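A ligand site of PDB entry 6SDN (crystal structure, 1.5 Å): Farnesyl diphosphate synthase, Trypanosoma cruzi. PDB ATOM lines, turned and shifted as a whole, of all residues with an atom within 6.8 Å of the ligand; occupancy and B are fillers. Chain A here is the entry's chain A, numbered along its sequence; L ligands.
The backbone NH of Thr 357 lies within hydrogen-bond range of an oxygen (O4) of the ligand (3.2 Å).
OG1 of Thr 54 is in hydrogen-bond range of O2 of the ligand, 2.4 Å away.
An oxygen (O1) of the ligand sits at hydrogen-bond distance from the backbone carbonyl oxygen (O) of Thr 212.
An oxygen (O4) of the ligand sits close to the side-chain hydroxyl of Thr 357 (3.4 Å).
The side-chain hydroxyl (OG1) of Thr 54 lies within hydrogen-bond range of the backbone carbonyl oxygen (O) of Phe 50.
The guanidinium group (NH2) of Arg 360 is in hydrogen-bond range of the backbone carbonyl oxygen (O) of Phe 246 (3.1 Å).
The side-chain hydroxyl of Thr 212 sits at hydrogen-bond distance from the guanidinium group of Arg 51.
The side-chain hydroxyl (OG1) of Thr 357 lies within hydrogen-bond range of the side-chain hydroxyl (OH) of Tyr 213 (2.8 Å).
OG1 of Thr 357 sits at hydrogen-bond distance from O of Val 353, at 2.9 Å.
O4 of the ligand lies close to O of Lys 356 (3.4 Å).
Merely in contact with the ligand: Tyr 213, Val 353, Phe 246, Phe 50, Arg 360 and Arg 51.
Hydrophobic or aromatic side chains within 4 Å of the ligand: Phe 50, Tyr 213, Phe 246 and Val 353.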
ATOM      1  N   PHE A  50      -4.697 -22.518 -29.898  1.00  0.00           N
ATOM      2  CA  PHE A  50      -5.150 -21.997 -28.604  1.00  0.00           C
ATOM      3  C   PHE A  50      -5.410 -23.127 -27.620  1.00  0.00           C
ATOM      4  O   PHE A  50      -5.040 -23.067 -26.441  1.00  0.00           O
ATOM      5  CB  PHE A  50      -6.454 -21.164 -28.723  1.00  0.00           C
ATOM      6  CG  PHE A  50      -6.316 -19.813 -29.371  1.00  0.00           C
ATOM      7  CD1 PHE A  50      -5.439 -18.859 -28.897  1.00  0.00           C
ATOM      8  CD2 PHE A  50      -7.164 -19.479 -30.413  1.00  0.00           C
ATOM      9  CE1 PHE A  50      -5.365 -17.617 -29.497  1.00  0.00           C
ATOM     10  CE2 PHE A  50      -7.106 -18.236 -31.009  1.00  0.00           C
ATOM     11  CZ  PHE A  50      -6.198 -17.305 -30.553  1.00  0.00           C
ATOM     12  N   ARG A  51      -6.118 -24.167 -28.068  1.00  0.00           N
ATOM     13  CA  ARG A  51      -6.525 -25.231 -27.164  1.00  0.00           C
ATOM     14  C   ARG A  51      -5.331 -26.026 -26.681  1.00  0.00           C
ATOM     15  O   ARG A  51      -5.146 -26.231 -25.473  1.00  0.00           O
ATOM     16  CB  ARG A  51      -7.532 -26.131 -27.872  1.00  0.00           C
ATOM     17  CG  ARG A  51      -8.820 -25.387 -28.216  1.00  0.00           C
ATOM     18  CD  ARG A  51      -9.661 -26.158 -29.225  1.00  0.00           C
ATOM     19  NE  ARG A  51     -10.858 -25.436 -29.656  1.00  0.00           N
ATOM     20  CZ  ARG A  51     -10.849 -24.435 -30.529  1.00  0.00           C
ATOM     21  NH1 ARG A  51     -11.976 -23.805 -30.851  1.00  0.00           N
ATOM     22  NH2 ARG A  51      -9.712 -24.011 -31.055  1.00  0.00           N
ATOM     23  N   GLY A  52      -4.492 -26.495 -27.599  1.00  0.00           N
ATOM     24  CA  GLY A  52      -3.336 -27.273 -27.180  1.00  0.00           C
ATOM     25  C   GLY A  52      -2.408 -26.485 -26.285  1.00  0.00           C
ATOM     26  O   GLY A  52      -1.881 -27.010 -25.292  1.00  0.00           O
ATOM     27  N   MET A  53      -2.142 -25.234 -26.649  1.00  0.00           N
ATOM     28  CA  MET A  53      -1.217 -24.427 -25.872  1.00  0.00           C
ATOM     29  C   MET A  53      -1.758 -24.075 -24.497  1.00  0.00           C
ATOM     30  O   MET A  53      -0.975 -23.808 -23.587  1.00  0.00           O
ATOM     31  CB  MET A  53      -0.861 -23.160 -26.641  1.00  0.00           C
ATOM     32  CG  MET A  53       0.084 -23.415 -27.797  1.00  0.00           C
ATOM     33  SD  MET A  53       1.714 -24.003 -27.306  1.00  0.00           S
ATOM     34  CE  MET A  53       2.257 -22.606 -26.317  1.00  0.00           C
ATOM     35  N   THR A  54      -3.078 -24.097 -24.304  1.00  0.00           N
ATOM     36  CA  THR A  54      -3.618 -23.903 -22.952  1.00  0.00           C
ATOM     37  C   THR A  54      -3.129 -24.999 -22.016  1.00  0.00           C
ATOM     38  O   THR A  54      -2.813 -24.726 -20.849  1.00  0.00           O
ATOM     39  CB  THR A  54      -5.140 -23.841 -23.003  1.00  0.00           C
ATOM     40  OG1 THR A  54      -5.505 -22.668 -23.751  1.00  0.00           O
ATOM     41  CG2 THR A  54      -5.721 -23.764 -21.611  1.00  0.00           C
ATOM     42  N   ASN A  57       0.408 -24.025 -21.149  1.00  0.00           N
ATOM     43  CA  ASN A  57       0.497 -22.844 -20.297  1.00  0.00           C
ATOM     44  C   ASN A  57       0.053 -23.142 -18.871  1.00  0.00           C
ATOM     45  O   ASN A  57       0.638 -22.620 -17.905  1.00  0.00           O
ATOM     46  CB  ASN A  57      -0.324 -21.717 -20.906  1.00  0.00           C
ATOM     47  CG  ASN A  57       0.239 -21.198 -22.208  1.00  0.00           C
ATOM     48  OD1 ASN A  57       1.453 -21.271 -22.458  1.00  0.00           O
ATOM     49  ND2 ASN A  57      -0.631 -20.663 -23.042  1.00  0.00           N
ATOM     50  N   TYR A 211     -14.758 -29.023 -25.372  1.00  0.00           N
ATOM     51  CA  TYR A 211     -13.471 -29.354 -25.990  1.00  0.00           C
ATOM     52  C   TYR A 211     -12.564 -28.138 -26.140  1.00  0.00           C
ATOM     53  O   TYR A 211     -11.347 -28.295 -26.190  1.00  0.00           O
ATOM     54  CB  TYR A 211     -13.673 -30.063 -27.347  1.00  0.00           C
ATOM     55  CG  TYR A 211     -13.738 -29.189 -28.597  1.00  0.00           C
ATOM     56  CD1 TYR A 211     -12.588 -28.857 -29.283  1.00  0.00           C
ATOM     57  CD2 TYR A 211     -14.941 -28.722 -29.095  1.00  0.00           C
ATOM     58  CE1 TYR A 211     -12.610 -28.088 -30.409  1.00  0.00           C
ATOM     59  CE2 TYR A 211     -14.971 -27.953 -30.227  1.00  0.00           C
ATOM     60  CZ  TYR A 211     -13.795 -27.640 -30.880  1.00  0.00           C
ATOM     61  OH  TYR A 211     -13.836 -26.836 -32.016  1.00  0.00           O
ATOM     62  N   THR A 212     -13.121 -26.925 -26.160  1.00  0.00           N
ATOM     63  CA  THR A 212     -12.328 -25.728 -26.391  1.00  0.00           C
ATOM     64  C   THR A 212     -11.758 -25.144 -25.094  1.00  0.00           C
ATOM     65  O   THR A 212     -10.646 -24.603 -25.131  1.00  0.00           O
ATOM     66  CB  THR A 212     -13.174 -24.698 -27.146  1.00  0.00           C
ATOM     67  OG1 THR A 212     -13.571 -25.275 -28.413  1.00  0.00           O
ATOM     68  CG2 THR A 212     -12.409 -23.408 -27.382  1.00  0.00           C
ATOM     69  N   TYR A 213     -12.475 -25.271 -23.974  1.00  0.00           N
ATOM     70  CA  TYR A 213     -12.013 -24.694 -22.705  1.00  0.00           C
ATOM     71  C   TYR A 213     -11.924 -25.683 -21.566  1.00  0.00           C
ATOM     72  O   TYR A 213     -10.902 -25.713 -20.861  1.00  0.00           O
ATOM     73  CB  TYR A 213     -12.903 -23.519 -22.287  1.00  0.00           C
ATOM     74  CG  TYR A 213     -12.690 -22.317 -23.178  1.00  0.00           C
ATOM     75  CD1 TYR A 213     -11.602 -21.473 -22.980  1.00  0.00           C
ATOM     76  CD2 TYR A 213     -13.530 -22.078 -24.252  1.00  0.00           C
ATOM     77  CE1 TYR A 213     -11.381 -20.392 -23.795  1.00  0.00           C
ATOM     78  CE2 TYR A 213     -13.296 -21.005 -25.082  1.00  0.00           C
ATOM     79  CZ  TYR A 213     -12.214 -20.181 -24.861  1.00  0.00           C
ATOM     80  OH  TYR A 213     -12.053 -19.108 -25.699  1.00  0.00           O
ATOM     81  N   LEU A 214     -12.932 -26.515 -21.341  1.00  0.00           N
ATOM     82  CA  LEU A 214     -12.860 -27.404 -20.189  1.00  0.00           C
ATOM     83  C   LEU A 214     -11.742 -28.420 -20.361  1.00  0.00           C
ATOM     84  O   LEU A 214     -10.890 -28.603 -19.470  1.00  0.00           O
ATOM     85  CB  LEU A 214     -14.203 -28.109 -19.942  1.00  0.00           C
ATOM     86  CG  LEU A 214     -14.186 -28.996 -18.697  1.00  0.00           C
ATOM     87  CD1 LEU A 214     -14.055 -28.152 -17.434  1.00  0.00           C
ATOM     88  CD2 LEU A 214     -15.435 -29.845 -18.638  1.00  0.00           C
ATOM     89  N   PRO A 216      -8.906 -28.479 -22.262  1.00  0.00           N
ATOM     90  CA  PRO A 216      -7.512 -27.998 -22.100  1.00  0.00           C
ATOM     91  C   PRO A 216      -7.175 -27.605 -20.678  1.00  0.00           C
ATOM     92  O   PRO A 216      -6.067 -27.903 -20.205  1.00  0.00           O
ATOM     93  CB  PRO A 216      -7.417 -26.797 -23.038  1.00  0.00           C
ATOM     94  CG  PRO A 216      -8.546 -26.912 -23.976  1.00  0.00           C
ATOM     95  CD  PRO A 216      -9.623 -27.743 -23.311  1.00  0.00           C
ATOM     96  N   LEU A 217      -8.090 -26.953 -19.959  1.00  0.00           N
ATOM     97  CA  LEU A 217      -7.809 -26.556 -18.579  1.00  0.00           C
ATOM     98  C   LEU A 217      -7.613 -27.778 -17.682  1.00  0.00           C
ATOM     99  O   LEU A 217      -6.643 -27.852 -16.916  1.00  0.00           O
ATOM    100  CB  LEU A 217      -8.929 -25.694 -18.033  1.00  0.00           C
ATOM    101  CG  LEU A 217      -9.008 -24.295 -18.651  1.00  0.00           C
ATOM    102  CD1 LEU A 217     -10.273 -23.585 -18.173  1.00  0.00           C
ATOM    103  CD2 LEU A 217      -7.768 -23.430 -18.339  1.00  0.00           C
ATOM    104  N   ILE A 242     -16.574 -18.639 -20.487  1.00  0.00           N
ATOM    105  CA  ILE A 242     -15.659 -18.153 -21.521  1.00  0.00           C
ATOM    106  C   ILE A 242     -15.998 -18.794 -22.864  1.00  0.00           C
ATOM    107  O   ILE A 242     -15.942 -18.142 -23.919  1.00  0.00           O
ATOM    108  CB  ILE A 242     -14.200 -18.404 -21.099  1.00  0.00           C
ATOM    109  CG1 ILE A 242     -13.858 -17.661 -19.811  1.00  0.00           C
ATOM    110  CG2 ILE A 242     -13.274 -17.969 -22.233  1.00  0.00           C
ATOM    111  CD1 ILE A 242     -12.475 -17.960 -19.301  1.00  0.00           C
ATOM    112  N   PHE A 246     -16.814 -17.069 -26.551  1.00  0.00           N
ATOM    113  CA  PHE A 246     -16.053 -17.396 -27.751  1.00  0.00           C
ATOM    114  C   PHE A 246     -16.981 -17.695 -28.919  1.00  0.00           C
ATOM    115  O   PHE A 246     -16.787 -17.206 -30.045  1.00  0.00           O
ATOM    116  CB  PHE A 246     -15.163 -18.612 -27.443  1.00  0.00           C
ATOM    117  CG  PHE A 246     -14.366 -19.121 -28.612  1.00  0.00           C
ATOM    118  CD1 PHE A 246     -13.091 -18.628 -28.861  1.00  0.00           C
ATOM    119  CD2 PHE A 246     -14.865 -20.115 -29.420  1.00  0.00           C
ATOM    120  CE1 PHE A 246     -12.339 -19.114 -29.921  1.00  0.00           C
ATOM    121  CE2 PHE A 246     -14.102 -20.603 -30.508  1.00  0.00           C
ATOM    122  CZ  PHE A 246     -12.858 -20.101 -30.737  1.00  0.00           C
ATOM    123  N   SER A 349      -3.714 -18.505 -14.713  1.00  0.00           N
ATOM    124  CA  SER A 349      -3.775 -19.167 -16.006  1.00  0.00           C
ATOM    125  C   SER A 349      -5.118 -18.937 -16.663  1.00  0.00           C
ATOM    126  O   SER A 349      -5.192 -18.684 -17.863  1.00  0.00           O
ATOM    127  CB  SER A 349      -3.486 -20.656 -15.847  1.00  0.00           C
ATOM    128  OG  SER A 349      -2.149 -20.834 -15.428  1.00  0.00           O
ATOM    129  N   VAL A 352      -5.288 -15.470 -18.048  1.00  0.00           N
ATOM    130  CA  VAL A 352      -4.601 -15.399 -19.342  1.00  0.00           C
ATOM    131  C   VAL A 352      -5.499 -15.928 -20.453  1.00  0.00           C
ATOM    132  O   VAL A 352      -5.588 -15.332 -21.537  1.00  0.00           O
ATOM    133  CB  VAL A 352      -3.273 -16.166 -19.284  1.00  0.00           C
ATOM    134  CG1 VAL A 352      -2.729 -16.402 -20.713  1.00  0.00           C
ATOM    135  CG2 VAL A 352      -2.293 -15.437 -18.413  1.00  0.00           C
ATOM    136  N   VAL A 353      -6.143 -17.071 -20.227  1.00  0.00           N
ATOM    137  CA  VAL A 353      -7.086 -17.624 -21.196  1.00  0.00           C
ATOM    138  C   VAL A 353      -8.166 -16.600 -21.551  1.00  0.00           C
ATOM    139  O   VAL A 353      -8.540 -16.440 -22.724  1.00  0.00           O
ATOM    140  CB  VAL A 353      -7.697 -18.919 -20.651  1.00  0.00           C
ATOM    141  CG1 VAL A 353      -8.916 -19.306 -21.454  1.00  0.00           C
ATOM    142  CG2 VAL A 353      -6.655 -20.053 -20.624  1.00  0.00           C
ATOM    143  N   TRP A 354      -8.727 -15.929 -20.537  1.00  0.00           N
ATOM    144  CA  TRP A 354      -9.791 -14.971 -20.814  1.00  0.00           C
ATOM    145  C   TRP A 354      -9.275 -13.794 -21.622  1.00  0.00           C
ATOM    146  O   TRP A 354      -9.898 -13.374 -22.606  1.00  0.00           O
ATOM    147  CB  TRP A 354     -10.442 -14.503 -19.520  1.00  0.00           C
ATOM    148  CG  TRP A 354     -11.344 -13.321 -19.722  1.00  0.00           C
ATOM    149  CD1 TRP A 354     -11.217 -12.092 -19.144  1.00  0.00           C
ATOM    150  CD2 TRP A 354     -12.480 -13.231 -20.590  1.00  0.00           C
ATOM    151  NE1 TRP A 354     -12.202 -11.253 -19.578  1.00  0.00           N
ATOM    152  CE2 TRP A 354     -12.990 -11.930 -20.473  1.00  0.00           C
ATOM    153  CE3 TRP A 354     -13.103 -14.129 -21.460  1.00  0.00           C
ATOM    154  CZ2 TRP A 354     -14.108 -11.502 -21.185  1.00  0.00           C
ATOM    155  CZ3 TRP A 354     -14.213 -13.700 -22.166  1.00  0.00           C
ATOM    156  CH2 TRP A 354     -14.701 -12.398 -22.029  1.00  0.00           C
ATOM    157  N   GLU A 355      -8.123 -13.241 -21.237  1.00  0.00           N
ATOM    158  CA  GLU A 355      -7.591 -12.088 -21.971  1.00  0.00           C
ATOM    159  C   GLU A 355      -7.385 -12.442 -23.435  1.00  0.00           C
ATOM    160  O   GLU A 355      -7.754 -11.663 -24.320  1.00  0.00           O
ATOM    161  CB  GLU A 355      -6.285 -11.603 -21.347  1.00  0.00           C
ATOM    162  CG  GLU A 355      -5.955 -10.153 -21.691  1.00  0.00           C
ATOM    163  N   LYS A 356      -6.787 -13.607 -23.705  1.00  0.00           N
ATOM    164  CA  LYS A 356      -6.587 -14.032 -25.081  1.00  0.00           C
ATOM    165  C   LYS A 356      -7.914 -14.150 -25.825  1.00  0.00           C
ATOM    166  O   LYS A 356      -8.037 -13.729 -26.980  1.00  0.00           O
ATOM    167  CB  LYS A 356      -5.847 -15.373 -25.123  1.00  0.00           C
ATOM    168  CG  LYS A 356      -4.354 -15.272 -24.914  1.00  0.00           C
ATOM    169  CD  LYS A 356      -3.694 -16.640 -24.863  1.00  0.00           C
ATOM    170  N   THR A 357      -8.931 -14.728 -25.168  1.00  0.00           N
ATOM    171  CA  THR A 357     -10.242 -14.857 -25.792  1.00  0.00           C
ATOM    172  C   THR A 357     -10.876 -13.498 -26.038  1.00  0.00           C
ATOM    173  O   THR A 357     -11.420 -13.250 -27.115  1.00  0.00           O
ATOM    174  CB  THR A 357     -11.157 -15.687 -24.888  1.00  0.00           C
ATOM    175  OG1 THR A 357     -10.575 -16.978 -24.695  1.00  0.00           O
ATOM    176  CG2 THR A 357     -12.513 -15.866 -25.519  1.00  0.00           C
ATOM    177  N   HIS A 358     -10.839 -12.631 -25.032  1.00  0.00           N
ATOM    178  CA  HIS A 358     -11.460 -11.316 -25.109  1.00  0.00           C
ATOM    179  C   HIS A 358     -10.861 -10.478 -26.230  1.00  0.00           C
ATOM    180  O   HIS A 358     -11.591  -9.786 -26.944  1.00  0.00           O
ATOM    181  CB  HIS A 358     -11.277 -10.629 -23.757  1.00  0.00           C
ATOM    182  CG  HIS A 358     -12.146  -9.437 -23.560  1.00  0.00           C
ATOM    183  ND1 HIS A 358     -11.893  -8.503 -22.577  1.00  0.00           N
ATOM    184  CD2 HIS A 358     -13.274  -9.030 -24.185  1.00  0.00           C
ATOM    185  CE1 HIS A 358     -12.824  -7.563 -22.611  1.00  0.00           C
ATOM    186  NE2 HIS A 358     -13.675  -7.862 -23.578  1.00  0.00           N
ATOM    187  N   LYS A 359      -9.544 -10.516 -26.372  1.00  0.00           N
ATOM    188  CA  LYS A 359      -8.806  -9.711 -27.346  1.00  0.00           C
ATOM    189  C   LYS A 359      -8.632 -10.409 -28.692  1.00  0.00           C
ATOM    190  O   LYS A 359      -7.774 -10.009 -29.475  1.00  0.00           O
ATOM    191  CB  LYS A 359      -7.434  -9.338 -26.776  1.00  0.00           C
ATOM    192  CG  LYS A 359      -7.494  -8.518 -25.491  1.00  0.00           C
ATOM    193  N   ARG A 360      -9.429 -11.441 -28.964  1.00  0.00           N
ATOM    194  CA  ARG A 360      -9.342 -12.153 -30.226  1.00  0.00           C
ATOM    195  C   ARG A 360      -9.872 -11.292 -31.357  1.00  0.00           C
ATOM    196  O   ARG A 360     -10.905 -10.625 -31.199  1.00  0.00           O
ATOM    197  CB  ARG A 360     -10.109 -13.467 -30.122  1.00  0.00           C
ATOM    198  CG  ARG A 360     -10.002 -14.380 -31.318  1.00  0.00           C
ATOM    199  CD  ARG A 360     -10.525 -15.763 -30.972  1.00  0.00           C
ATOM    200  NE  ARG A 360     -11.977 -15.786 -30.735  1.00  0.00           N
ATOM    201  CZ  ARG A 360     -12.875 -16.199 -31.628  1.00  0.00           C
ATOM    202  NH1 ARG A 360     -12.492 -16.592 -32.836  1.00  0.00           N
ATOM    203  NH2 ARG A 360     -14.174 -16.212 -31.322  1.00  0.00           N
HETATM  204  C1  LIG L   1      -8.613 -21.673 -25.377  1.00  0.00           C
HETATM  205  C2  LIG L   1      -7.830 -20.603 -24.970  1.00  0.00           C
HETATM  206  C3  LIG L   1      -7.866 -19.401 -25.654  1.00  0.00           C
HETATM  207  C4  LIG L   1      -8.721 -19.291 -26.749  1.00  0.00           C
HETATM  208  C5  LIG L   1      -9.501 -20.335 -27.176  1.00  0.00           C
HETATM  209  C6  LIG L   1      -9.449 -21.537 -26.495  1.00  0.00           C
HETATM  210  O1  LIG L   1      -8.542 -22.839 -24.674  1.00  0.00           O
HETATM  211  O2  LIG L   1      -7.037 -20.761 -23.878  1.00  0.00           O
HETATM  212  N1  LIG L   1      -8.838 -17.979 -27.393  1.00  0.00           N
HETATM  213  O3  LIG L   1      -9.703 -17.836 -28.253  1.00  0.00           O
HETATM  214  O4  LIG L   1      -8.073 -17.098 -27.060  1.00  0.00           O
